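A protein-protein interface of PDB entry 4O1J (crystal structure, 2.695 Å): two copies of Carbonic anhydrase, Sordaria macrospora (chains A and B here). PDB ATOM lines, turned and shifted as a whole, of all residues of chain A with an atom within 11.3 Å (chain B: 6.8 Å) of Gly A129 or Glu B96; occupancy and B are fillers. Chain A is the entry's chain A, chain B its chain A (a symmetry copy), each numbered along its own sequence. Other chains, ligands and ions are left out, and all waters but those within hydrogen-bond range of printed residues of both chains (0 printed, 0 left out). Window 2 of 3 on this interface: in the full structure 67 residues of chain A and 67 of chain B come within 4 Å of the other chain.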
ATOM      1  N   SER A  57       4.616 -12.323  21.487  1.00  0.00           N
ATOM      2  CA  SER A  57       5.583 -12.568  22.548  1.00  0.00           C
ATOM      3  C   SER A  57       5.823 -11.342  23.421  1.00  0.00           C
ATOM      4  O   SER A  57       6.383 -11.460  24.514  1.00  0.00           O
ATOM      5  CB  SER A  57       6.913 -13.022  21.929  1.00  0.00           C
ATOM      6  OG  SER A  57       6.864 -14.384  21.542  1.00  0.00           O
ATOM      7  N   ASN A  79       4.195 -16.030  19.884  1.00  0.00           N
ATOM      8  CA  ASN A  79       5.369 -15.863  19.038  1.00  0.00           C
ATOM      9  C   ASN A  79       5.518 -14.418  18.592  1.00  0.00           C
ATOM     10  O   ASN A  79       4.754 -13.549  19.010  1.00  0.00           O
ATOM     11  CB  ASN A  79       5.302 -16.793  17.827  1.00  0.00           C
ATOM     12  CG  ASN A  79       4.071 -16.559  16.974  1.00  0.00           C
ATOM     13  OD1 ASN A  79       3.858 -15.465  16.439  1.00  0.00           O
ATOM     14  ND2 ASN A  79       3.267 -17.603  16.813  1.00  0.00           N
ATOM     15  N   ILE A  80       6.504 -14.159  17.742  1.00  0.00           N
ATOM     16  CA  ILE A  80       6.706 -12.814  17.227  1.00  0.00           C
ATOM     17  C   ILE A  80       5.526 -12.358  16.370  1.00  0.00           C
ATOM     18  O   ILE A  80       5.213 -12.978  15.356  1.00  0.00           O
ATOM     19  CB  ILE A  80       8.002 -12.717  16.414  1.00  0.00           C
ATOM     20  CG1 ILE A  80       9.199 -12.990  17.326  1.00  0.00           C
ATOM     21  CG2 ILE A  80       8.133 -11.337  15.775  1.00  0.00           C
ATOM     22  CD1 ILE A  80       9.277 -12.070  18.538  1.00  0.00           C
ATOM     23  N   GLY A 116       6.207  -4.620  17.453  1.00  0.00           N
ATOM     24  CA  GLY A 116       7.512  -4.459  16.846  1.00  0.00           C
ATOM     25  C   GLY A 116       7.640  -5.215  15.541  1.00  0.00           C
ATOM     26  O   GLY A 116       8.300  -4.746  14.617  1.00  0.00           O
ATOM     27  N   GLY A 117       7.005  -6.385  15.467  1.00  0.00           N
ATOM     28  CA  GLY A 117       7.046  -7.199  14.267  1.00  0.00           C
ATOM     29  C   GLY A 117       6.287  -6.524  13.148  1.00  0.00           C
ATOM     30  O   GLY A 117       6.712  -6.549  11.992  1.00  0.00           O
ATOM     31  N   GLY A 125      13.940  -2.248   5.390  1.00  0.00           N
ATOM     32  CA  GLY A 125      15.292  -2.722   5.605  1.00  0.00           C
ATOM     33  C   GLY A 125      15.284  -4.185   5.990  1.00  0.00           C
ATOM     34  O   GLY A 125      14.254  -4.716   6.398  1.00  0.00           O
ATOM     35  N   ARG A 126      16.425  -4.846   5.846  1.00  0.00           N
ATOM     36  CA  ARG A 126      16.552  -6.206   6.338  1.00  0.00           C
ATOM     37  C   ARG A 126      16.623  -6.159   7.852  1.00  0.00           C
ATOM     38  O   ARG A 126      17.469  -5.473   8.422  1.00  0.00           O
ATOM     39  CB  ARG A 126      17.790  -6.890   5.760  1.00  0.00           C
ATOM     40  CG  ARG A 126      17.698  -7.150   4.270  1.00  0.00           C
ATOM     41  CD  ARG A 126      18.329  -8.476   3.876  1.00  0.00           C
ATOM     42  NE  ARG A 126      17.405  -9.597   4.041  1.00  0.00           N
ATOM     43  CZ  ARG A 126      17.531 -10.770   3.424  1.00  0.00           C
ATOM     44  NH1 ARG A 126      18.541 -10.980   2.588  1.00  0.00           N
ATOM     45  NH2 ARG A 126      16.644 -11.735   3.637  1.00  0.00           N
ATOM     46  N   ILE A 127      15.725  -6.883   8.505  1.00  0.00           N
ATOM     47  CA  ILE A 127      15.751  -6.969   9.958  1.00  0.00           C
ATOM     48  C   ILE A 127      16.876  -7.910  10.379  1.00  0.00           C
ATOM     49  O   ILE A 127      17.391  -7.827  11.495  1.00  0.00           O
ATOM     50  CB  ILE A 127      14.400  -7.440  10.511  1.00  0.00           C
ATOM     51  CG1 ILE A 127      13.296  -6.514  10.001  1.00  0.00           C
ATOM     52  CG2 ILE A 127      14.407  -7.461  12.031  1.00  0.00           C
ATOM     53  CD1 ILE A 127      11.927  -6.892  10.473  1.00  0.00           C
ATOM     54  N   GLY A 128      17.266  -8.790   9.461  1.00  0.00           N
ATOM     55  CA  GLY A 128      18.372  -9.698   9.696  1.00  0.00           C
ATOM     56  C   GLY A 128      17.976 -11.033  10.295  1.00  0.00           C
ATOM     57  O   GLY A 128      16.881 -11.198  10.847  1.00  0.00           O
ATOM     58  N   GLY A 129      18.888 -11.994  10.175  1.00  0.00           N
ATOM     59  CA  GLY A 129      18.679 -13.337  10.675  1.00  0.00           C
ATOM     60  C   GLY A 129      17.450 -13.999  10.094  1.00  0.00           C
ATOM     61  O   GLY A 129      17.135 -13.873   8.909  1.00  0.00           O
ATOM     62  N   VAL A 130      16.759 -14.719  10.962  1.00  0.00           N
ATOM     63  CA  VAL A 130      15.580 -15.492  10.612  1.00  0.00           C
ATOM     64  C   VAL A 130      14.315 -14.632  10.479  1.00  0.00           C
ATOM     65  O   VAL A 130      13.335 -15.049   9.857  1.00  0.00           O
ATOM     66  CB  VAL A 130      15.374 -16.605  11.665  1.00  0.00           C
ATOM     67  CG1 VAL A 130      14.048 -16.453  12.418  1.00  0.00           C
ATOM     68  CG2 VAL A 130      15.529 -17.974  11.029  1.00  0.00           C
ATOM     69  N   LEU A 131      14.360 -13.426  11.044  1.00  0.00           N
ATOM     70  CA  LEU A 131      13.171 -12.584  11.217  1.00  0.00           C
ATOM     71  C   LEU A 131      12.455 -12.150   9.934  1.00  0.00           C
ATOM     72  O   LEU A 131      11.237 -12.026   9.927  1.00  0.00           O
ATOM     73  CB  LEU A 131      13.543 -11.345  12.037  1.00  0.00           C
ATOM     74  CG  LEU A 131      13.721 -11.626  13.535  1.00  0.00           C
ATOM     75  CD1 LEU A 131      14.654 -10.624  14.197  1.00  0.00           C
ATOM     76  CD2 LEU A 131      12.370 -11.625  14.233  1.00  0.00           C
ATOM     77  N   ASP A 132      13.189 -11.911   8.856  1.00  0.00           N
ATOM     78  CA  ASP A 132      12.548 -11.534   7.597  1.00  0.00           C
ATOM     79  C   ASP A 132      11.679 -12.676   7.062  1.00  0.00           C
ATOM     80  O   ASP A 132      10.593 -12.455   6.507  1.00  0.00           O
ATOM     81  CB  ASP A 132      13.606 -11.132   6.576  1.00  0.00           C
ATOM     82  CG  ASP A 132      14.503 -10.020   7.088  1.00  0.00           C
ATOM     83  OD1 ASP A 132      14.218  -8.831   6.814  1.00  0.00           O
ATOM     84  OD2 ASP A 132      15.488 -10.342   7.786  1.00  0.00           O
ATOM     85  N   THR A 133      12.132 -13.901   7.301  1.00  0.00           N
ATOM     86  CA  THR A 133      11.406 -15.082   6.870  1.00  0.00           C
ATOM     87  C   THR A 133      10.186 -15.320   7.746  1.00  0.00           C
ATOM     88  O   THR A 133       9.108 -15.623   7.237  1.00  0.00           O
ATOM     89  CB  THR A 133      12.311 -16.338   6.896  1.00  0.00           C
ATOM     90  OG1 THR A 133      13.420 -16.149   6.007  1.00  0.00           O
ATOM     91  CG2 THR A 133      11.538 -17.577   6.470  1.00  0.00           C
ATOM     92  N   TRP A 134      10.338 -15.153   9.054  1.00  0.00           N
ATOM     93  CA  TRP A 134       9.202 -15.341   9.950  1.00  0.00           C
ATOM     94  C   TRP A 134       8.138 -14.282   9.683  1.00  0.00           C
ATOM     95  O   TRP A 134       6.946 -14.587   9.646  1.00  0.00           O
ATOM     96  CB  TRP A 134       9.631 -15.295  11.418  1.00  0.00           C
ATOM     97  CG  TRP A 134       8.457 -15.358  12.357  1.00  0.00           C
ATOM     98  CD1 TRP A 134       7.919 -14.319  13.068  1.00  0.00           C
ATOM     99  CD2 TRP A 134       7.646 -16.502  12.649  1.00  0.00           C
ATOM    100  NE1 TRP A 134       6.840 -14.753  13.798  1.00  0.00           N
ATOM    101  CE2 TRP A 134       6.648 -16.094  13.558  1.00  0.00           C
ATOM    102  CE3 TRP A 134       7.671 -17.843  12.239  1.00  0.00           C
ATOM    103  CZ2 TRP A 134       5.688 -16.966  14.063  1.00  0.00           C
ATOM    104  CZ3 TRP A 134       6.713 -18.712  12.737  1.00  0.00           C
ATOM    105  CH2 TRP A 134       5.734 -18.268  13.639  1.00  0.00           C
ATOM    106  N   LEU A 135       8.583 -13.050   9.462  1.00  0.00           N
ATOM    107  CA  LEU A 135       7.675 -11.940   9.214  1.00  0.00           C
ATOM    108  C   LEU A 135       7.195 -11.872   7.774  1.00  0.00           C
ATOM    109  O   LEU A 135       6.424 -10.976   7.427  1.00  0.00           O
ATOM    110  CB  LEU A 135       8.343 -10.616   9.582  1.00  0.00           C
ATOM    111  CG  LEU A 135       8.523 -10.362  11.077  1.00  0.00           C
ATOM    112  CD1 LEU A 135       9.270  -9.067  11.291  1.00  0.00           C
ATOM    113  CD2 LEU A 135       7.171 -10.338  11.781  1.00  0.00           C
ATOM    114  N   LEU A 136       7.644 -12.803   6.935  1.00  0.00           N
ATOM    115  CA  LEU A 136       7.253 -12.773   5.525  1.00  0.00           C
ATOM    116  C   LEU A 136       5.732 -12.748   5.281  1.00  0.00           C
ATOM    117  O   LEU A 136       5.279 -12.000   4.414  1.00  0.00           O
ATOM    118  CB  LEU A 136       7.869 -13.953   4.770  1.00  0.00           C
ATOM    119  CG  LEU A 136       7.867 -13.688   3.266  1.00  0.00           C
ATOM    120  CD1 LEU A 136       8.641 -12.413   2.963  1.00  0.00           C
ATOM    121  CD2 LEU A 136       8.445 -14.855   2.499  1.00  0.00           C
ATOM    122  N   LEU B  52      13.649 -13.145  28.860  1.00  0.00           N
ATOM    123  CA  LEU B  52      12.974 -13.973  27.876  1.00  0.00           C
ATOM    124  C   LEU B  52      12.592 -15.268  28.571  1.00  0.00           C
ATOM    125  O   LEU B  52      13.438 -15.936  29.149  1.00  0.00           O
ATOM    126  CB  LEU B  52      13.872 -14.247  26.663  1.00  0.00           C
ATOM    127  CG  LEU B  52      13.543 -15.441  25.748  1.00  0.00           C
ATOM    128  CD1 LEU B  52      12.145 -15.355  25.141  1.00  0.00           C
ATOM    129  CD2 LEU B  52      14.590 -15.558  24.652  1.00  0.00           C
ATOM    130  N   THR B  91      10.572 -20.471  17.253  1.00  0.00           N
ATOM    131  CA  THR B  91      11.254 -20.208  18.517  1.00  0.00           C
ATOM    132  C   THR B  91      12.468 -19.311  18.286  1.00  0.00           C
ATOM    133  O   THR B  91      12.726 -18.369  19.050  1.00  0.00           O
ATOM    134  CB  THR B  91      11.706 -21.528  19.207  1.00  0.00           C
ATOM    135  OG1 THR B  91      10.588 -22.419  19.343  1.00  0.00           O
ATOM    136  CG2 THR B  91      12.275 -21.255  20.582  1.00  0.00           C
ATOM    137  N   THR B  92      13.182 -19.586  17.198  1.00  0.00           N
ATOM    138  CA  THR B  92      14.408 -18.870  16.868  1.00  0.00           C
ATOM    139  C   THR B  92      14.131 -17.400  16.587  1.00  0.00           C
ATOM    140  O   THR B  92      14.976 -16.542  16.844  1.00  0.00           O
ATOM    141  CB  THR B  92      15.102 -19.493  15.642  1.00  0.00           C
ATOM    142  OG1 THR B  92      15.310 -20.892  15.878  1.00  0.00           O
ATOM    143  CG2 THR B  92      16.446 -18.809  15.364  1.00  0.00           C
ATOM    144  N   ALA B  93      12.941 -17.108  16.072  1.00  0.00           N
ATOM    145  CA  ALA B  93      12.550 -15.722  15.845  1.00  0.00           C
ATOM    146  C   ALA B  93      12.377 -14.973  17.170  1.00  0.00           C
ATOM    147  O   ALA B  93      12.836 -13.833  17.312  1.00  0.00           O
ATOM    148  CB  ALA B  93      11.271 -15.662  15.028  1.00  0.00           C
ATOM    149  N   VAL B  94      11.740 -15.623  18.142  1.00  0.00           N
ATOM    150  CA  VAL B  94      11.508 -15.001  19.442  1.00  0.00           C
ATOM    151  C   VAL B  94      12.836 -14.776  20.143  1.00  0.00           C
ATOM    152  O   VAL B  94      13.073 -13.709  20.711  1.00  0.00           O
ATOM    153  CB  VAL B  94      10.592 -15.856  20.353  1.00  0.00           C
ATOM    154  CG1 VAL B  94      10.448 -15.202  21.708  1.00  0.00           C
ATOM    155  CG2 VAL B  94       9.225 -16.060  19.710  1.00  0.00           C
ATOM    156  N   ILE B  95      13.708 -15.778  20.077  1.00  0.00           N
ATOM    157  CA  ILE B  95      15.036 -15.663  20.665  1.00  0.00           C
ATOM    158  C   ILE B  95      15.843 -14.546  20.010  1.00  0.00           C
ATOM    159  O   ILE B  95      16.470 -13.741  20.703  1.00  0.00           O
ATOM    160  CB  ILE B  95      15.818 -16.972  20.553  1.00  0.00           C
ATOM    161  CG1 ILE B  95      15.117 -18.085  21.334  1.00  0.00           C
ATOM    162  CG2 ILE B  95      17.246 -16.788  21.058  1.00  0.00           C
ATOM    163  CD1 ILE B  95      15.748 -19.440  21.143  1.00  0.00           C
ATOM    164  N   GLU B  96      15.824 -14.485  18.680  1.00  0.00           N
ATOM    165  CA  GLU B  96      16.578 -13.448  17.987  1.00  0.00           C
ATOM    166  C   GLU B  96      16.085 -12.059  18.344  1.00  0.00           C
ATOM    167  O   GLU B  96      16.888 -11.163  18.597  1.00  0.00           O
ATOM    168  CB  GLU B  96      16.512 -13.611  16.469  1.00  0.00           C
ATOM    169  CG  GLU B  96      17.793 -14.128  15.848  1.00  0.00           C
ATOM    170  CD  GLU B  96      17.625 -14.498  14.381  1.00  0.00           C
ATOM    171  OE1 GLU B  96      18.221 -15.506  13.938  1.00  0.00           O
ATOM    172  OE2 GLU B  96      16.913 -13.755  13.667  1.00  0.00           O
ATOM    173  N   TYR B  97      14.765 -11.884  18.376  1.00  0.00           N
ATOM    174  CA  TYR B  97      14.200 -10.574  18.677  1.00  0.00           C
ATOM    175  C   TYR B  97      14.490 -10.179  20.123  1.00  0.00           C
ATOM    176  O   TYR B  97      14.802  -9.020  20.412  1.00  0.00           O
ATOM    177  CB  TYR B  97      12.696 -10.554  18.422  1.00  0.00           C
ATOM    178  CG  TYR B  97      12.142  -9.156  18.288  1.00  0.00           C
ATOM    179  CD1 TYR B  97      12.147  -8.509  17.059  1.00  0.00           C
ATOM    180  CD2 TYR B  97      11.629  -8.471  19.388  1.00  0.00           C
ATOM    181  CE1 TYR B  97      11.649  -7.226  16.920  1.00  0.00           C
ATOM    182  CE2 TYR B  97      11.130  -7.179  19.261  1.00  0.00           C
ATOM    183  CZ  TYR B  97      11.142  -6.563  18.021  1.00  0.00           C
ATOM    184  OH  TYR B  97      10.652  -5.283  17.869  1.00  0.00           O
ATOM    185  N   ALA B  98      14.409 -11.154  21.023  1.00  0.00           N
ATOM    186  CA  ALA B  98      14.617 -10.905  22.445  1.00  0.00           C
ATOM    187  C   ALA B  98      16.072 -10.556  22.755  1.00  0.00           C
ATOM    188  O   ALA B  98      16.346  -9.656  23.548  1.00  0.00           O
ATOM    189  CB  ALA B  98      14.181 -12.113  23.257  1.00  0.00           C
ATOM    190  N   VAL B  99      17.000 -11.260  22.118  1.00  0.00           N
ATOM    191  CA  VAL B  99      18.411 -11.129  22.454  1.00  0.00           C
ATOM    192  C   VAL B  99      19.090 -10.004  21.673  1.00  0.00           C
ATOM    193  O   VAL B  99      19.878  -9.247  22.233  1.00  0.00           O
ATOM    194  CB  VAL B  99      19.169 -12.457  22.203  1.00  0.00           C
ATOM    195  CG1 VAL B  99      20.668 -12.266  22.380  1.00  0.00           C
ATOM    196  CG2 VAL B  99      18.665 -13.547  23.146  1.00  0.00           C
ATOM    197  N   ALA B 100      18.771  -9.873  20.391  1.00  0.00           N
ATOM    198  CA  ALA B 100      19.471  -8.902  19.551  1.00  0.00           C
ATOM    199  C   ALA B 100      18.778  -7.531  19.448  1.00  0.00           C
ATOM    200  O   ALA B 100      19.415  -6.541  19.084  1.00  0.00           O
ATOM    201  CB  ALA B 100      19.680  -9.483  18.157  1.00  0.00           C
ATOM    202  N   HIS B 101      17.495  -7.460  19.781  1.00  0.00           N
ATOM    203  CA  HIS B 101      16.765  -6.205  19.613  1.00  0.00           C
ATOM    204  C   HIS B 101      16.364  -5.578  20.938  1.00  0.00           C
ATOM    205  O   HIS B 101      16.538  -4.372  21.139  1.00  0.00           O
ATOM    206  CB  HIS B 101      15.522  -6.419  18.744  1.00  0.00           C
ATOM    207  CG  HIS B 101      15.837  -6.701  17.309  1.00  0.00           C
ATOM    208  ND1 HIS B 101      16.406  -7.884  16.891  1.00  0.00           N
ATOM    209  CD2 HIS B 101      15.689  -5.940  16.200  1.00  0.00           C
ATOM    210  CE1 HIS B 101      16.587  -7.842  15.581  1.00  0.00           C
ATOM    211  NE2 HIS B 101      16.161  -6.674  15.138  1.00  0.00           N
ATOM    212  N   LEU B 102      15.835  -6.398  21.837  1.00  0.00           N
ATOM    213  CA  LEU B 102      15.401  -5.929  23.148  1.00  0.00           C
ATOM    214  C   LEU B 102      16.535  -5.980  24.176  1.00  0.00           C
ATOM    215  O   LEU B 102      16.472  -5.332  25.224  1.00  0.00           O
ATOM    216  CB  LEU B 102      14.213  -6.759  23.623  1.00  0.00           C
ATOM    217  CG  LEU B 102      12.942  -6.544  22.798  1.00  0.00           C
ATOM    218  CD1 LEU B 102      11.801  -7.388  23.336  1.00  0.00           C
ATOM    219  CD2 LEU B 102      12.568  -5.074  22.779  1.00  0.00           C
ATOM    220  N   ASN B 177      22.989 -22.020  20.359  1.00  0.00           N
ATOM    221  CA  ASN B 177      22.448 -20.964  19.512  1.00  0.00           C
ATOM    222  C   ASN B 177      23.472 -19.846  19.335  1.00  0.00           C
ATOM    223  O   ASN B 177      24.053 -19.381  20.313  1.00  0.00           O
ATOM    224  CB  ASN B 177      21.166 -20.410  20.119  1.00  0.00           C
ATOM    225  CG  ASN B 177      20.519 -19.353  19.258  1.00  0.00           C
ATOM    226  OD1 ASN B 177      21.014 -18.232  19.145  1.00  0.00           O
ATOM    227  ND2 ASN B 177      19.379 -19.693  18.675  1.00  0.00           N
ATOM    228  N   THR B 179      23.231 -16.568  18.394  1.00  0.00           N
ATOM    229  CA  THR B 179      22.897 -15.258  18.934  1.00  0.00           C
ATOM    230  C   THR B 179      23.079 -15.234  20.444  1.00  0.00           C
ATOM    231  O   THR B 179      23.584 -14.262  21.025  1.00  0.00           O
ATOM    232  CB  THR B 179      21.447 -14.872  18.608  1.00  0.00           C
ATOM    233  OG1 THR B 179      21.207 -15.034  17.203  1.00  0.00           O
ATOM    234  CG2 THR B 179      21.180 -13.431  19.013  1.00  0.00           C
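The side-chain carboxylate (OE2) of Glu B96 lies within hydrogen-bond range of the backbone NH (N) of Val A130, 2.9 Å away.
The backbone carbonyl oxygen (O) of Asn A79 is in hydrogen-bond range of the backbone NH (N) of Ser A57 (2.8 Å).
The backbone carbonyl oxygen (O) of Ile A80 sits at hydrogen-bond distance from the indole nitrogen (NE1) of Trp A134.
N of Ile A127 sits at hydrogen-bond distance from OD1 of Asp A132 (3.0 Å).
The backbone NH (N) of Gly A128 sits at hydrogen-bond distance from the side-chain carboxylate (OD2) of Asp A132 (2.9 Å).
N of Leu B102 is in hydrogen-bond range of O of Tyr B97 (3.2 Å).
Among the printed residues, pairs that only touch across the chains: Gly A116 with Tyr B97, Ser A57 with Val B94, Gly A129 with Glu B96, Ile A127 with His B101, Leu A131 with His B101, Leu A131 with Glu B96, Ile A80 with Val B94, Ile A80 with Ala B93, Ile A80 with Tyr B97, Gly A128 with Glu B96, Val A130 with Ala B93, Leu A131 with Ala B93, Trp A134 with Ala B93 and Asn A79 with Val B94.
Of the printed residues of chain B, Gly A116 touches Tyr B97.
Gly A125 touches none of the printed residues of chain B.
Arg A126 touches none of the printed residues of chain B.
Of the printed residues of chain B, Gly A128 touches Glu B96.
No residue of chain A comes within 4 Å of Thr B92.
Ala B93 touches just these residues of chain A: Ile A80 (3.7 Å), Val A130 (3.8 Å), Leu A131 (3.8 Å) and Trp A134 (3.9 Å).
Val B94 touches three residues of chain A.
No residue of chain A comes within 4 Å of Ile B95.
Of chain A, only Gly A128, Gly A129, Val A130 and Leu A131 come within 4 Å of Glu B96.
Of the printed residues of chain A, Tyr B97 touches Ile A80 (3.7 Å) and Gly A116 (3.4 Å).
No residue of chain A comes within 4 Å of Val B99.
Hydrophobic or aromatic side chains of chain B within 4 Å of the printed part of chain A: Ala B93, Val B94, Tyr B97 and His B101.
Of the 17 printed residues of chain A, 10 touch a printed residue of chain B.
Hydrophobic or aromatic side chains of chain A within 4 Å of the printed part of chain B: Ile A80, Ile A127, Val A130, Leu A131 and Trp A134.
Along chain A the printed residues that touch a printed residue of chain B span positions 57 to 134.
Among the printed residues, no Asp or Glu carboxylate lies within 4 Å of a Lys or Arg side-chain nitrogen of the other chain.
No position is printed for both chains.
Of the 15 pairs that touch across the chains among the printed residues, none has its exchanged pair printed and touching as well.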
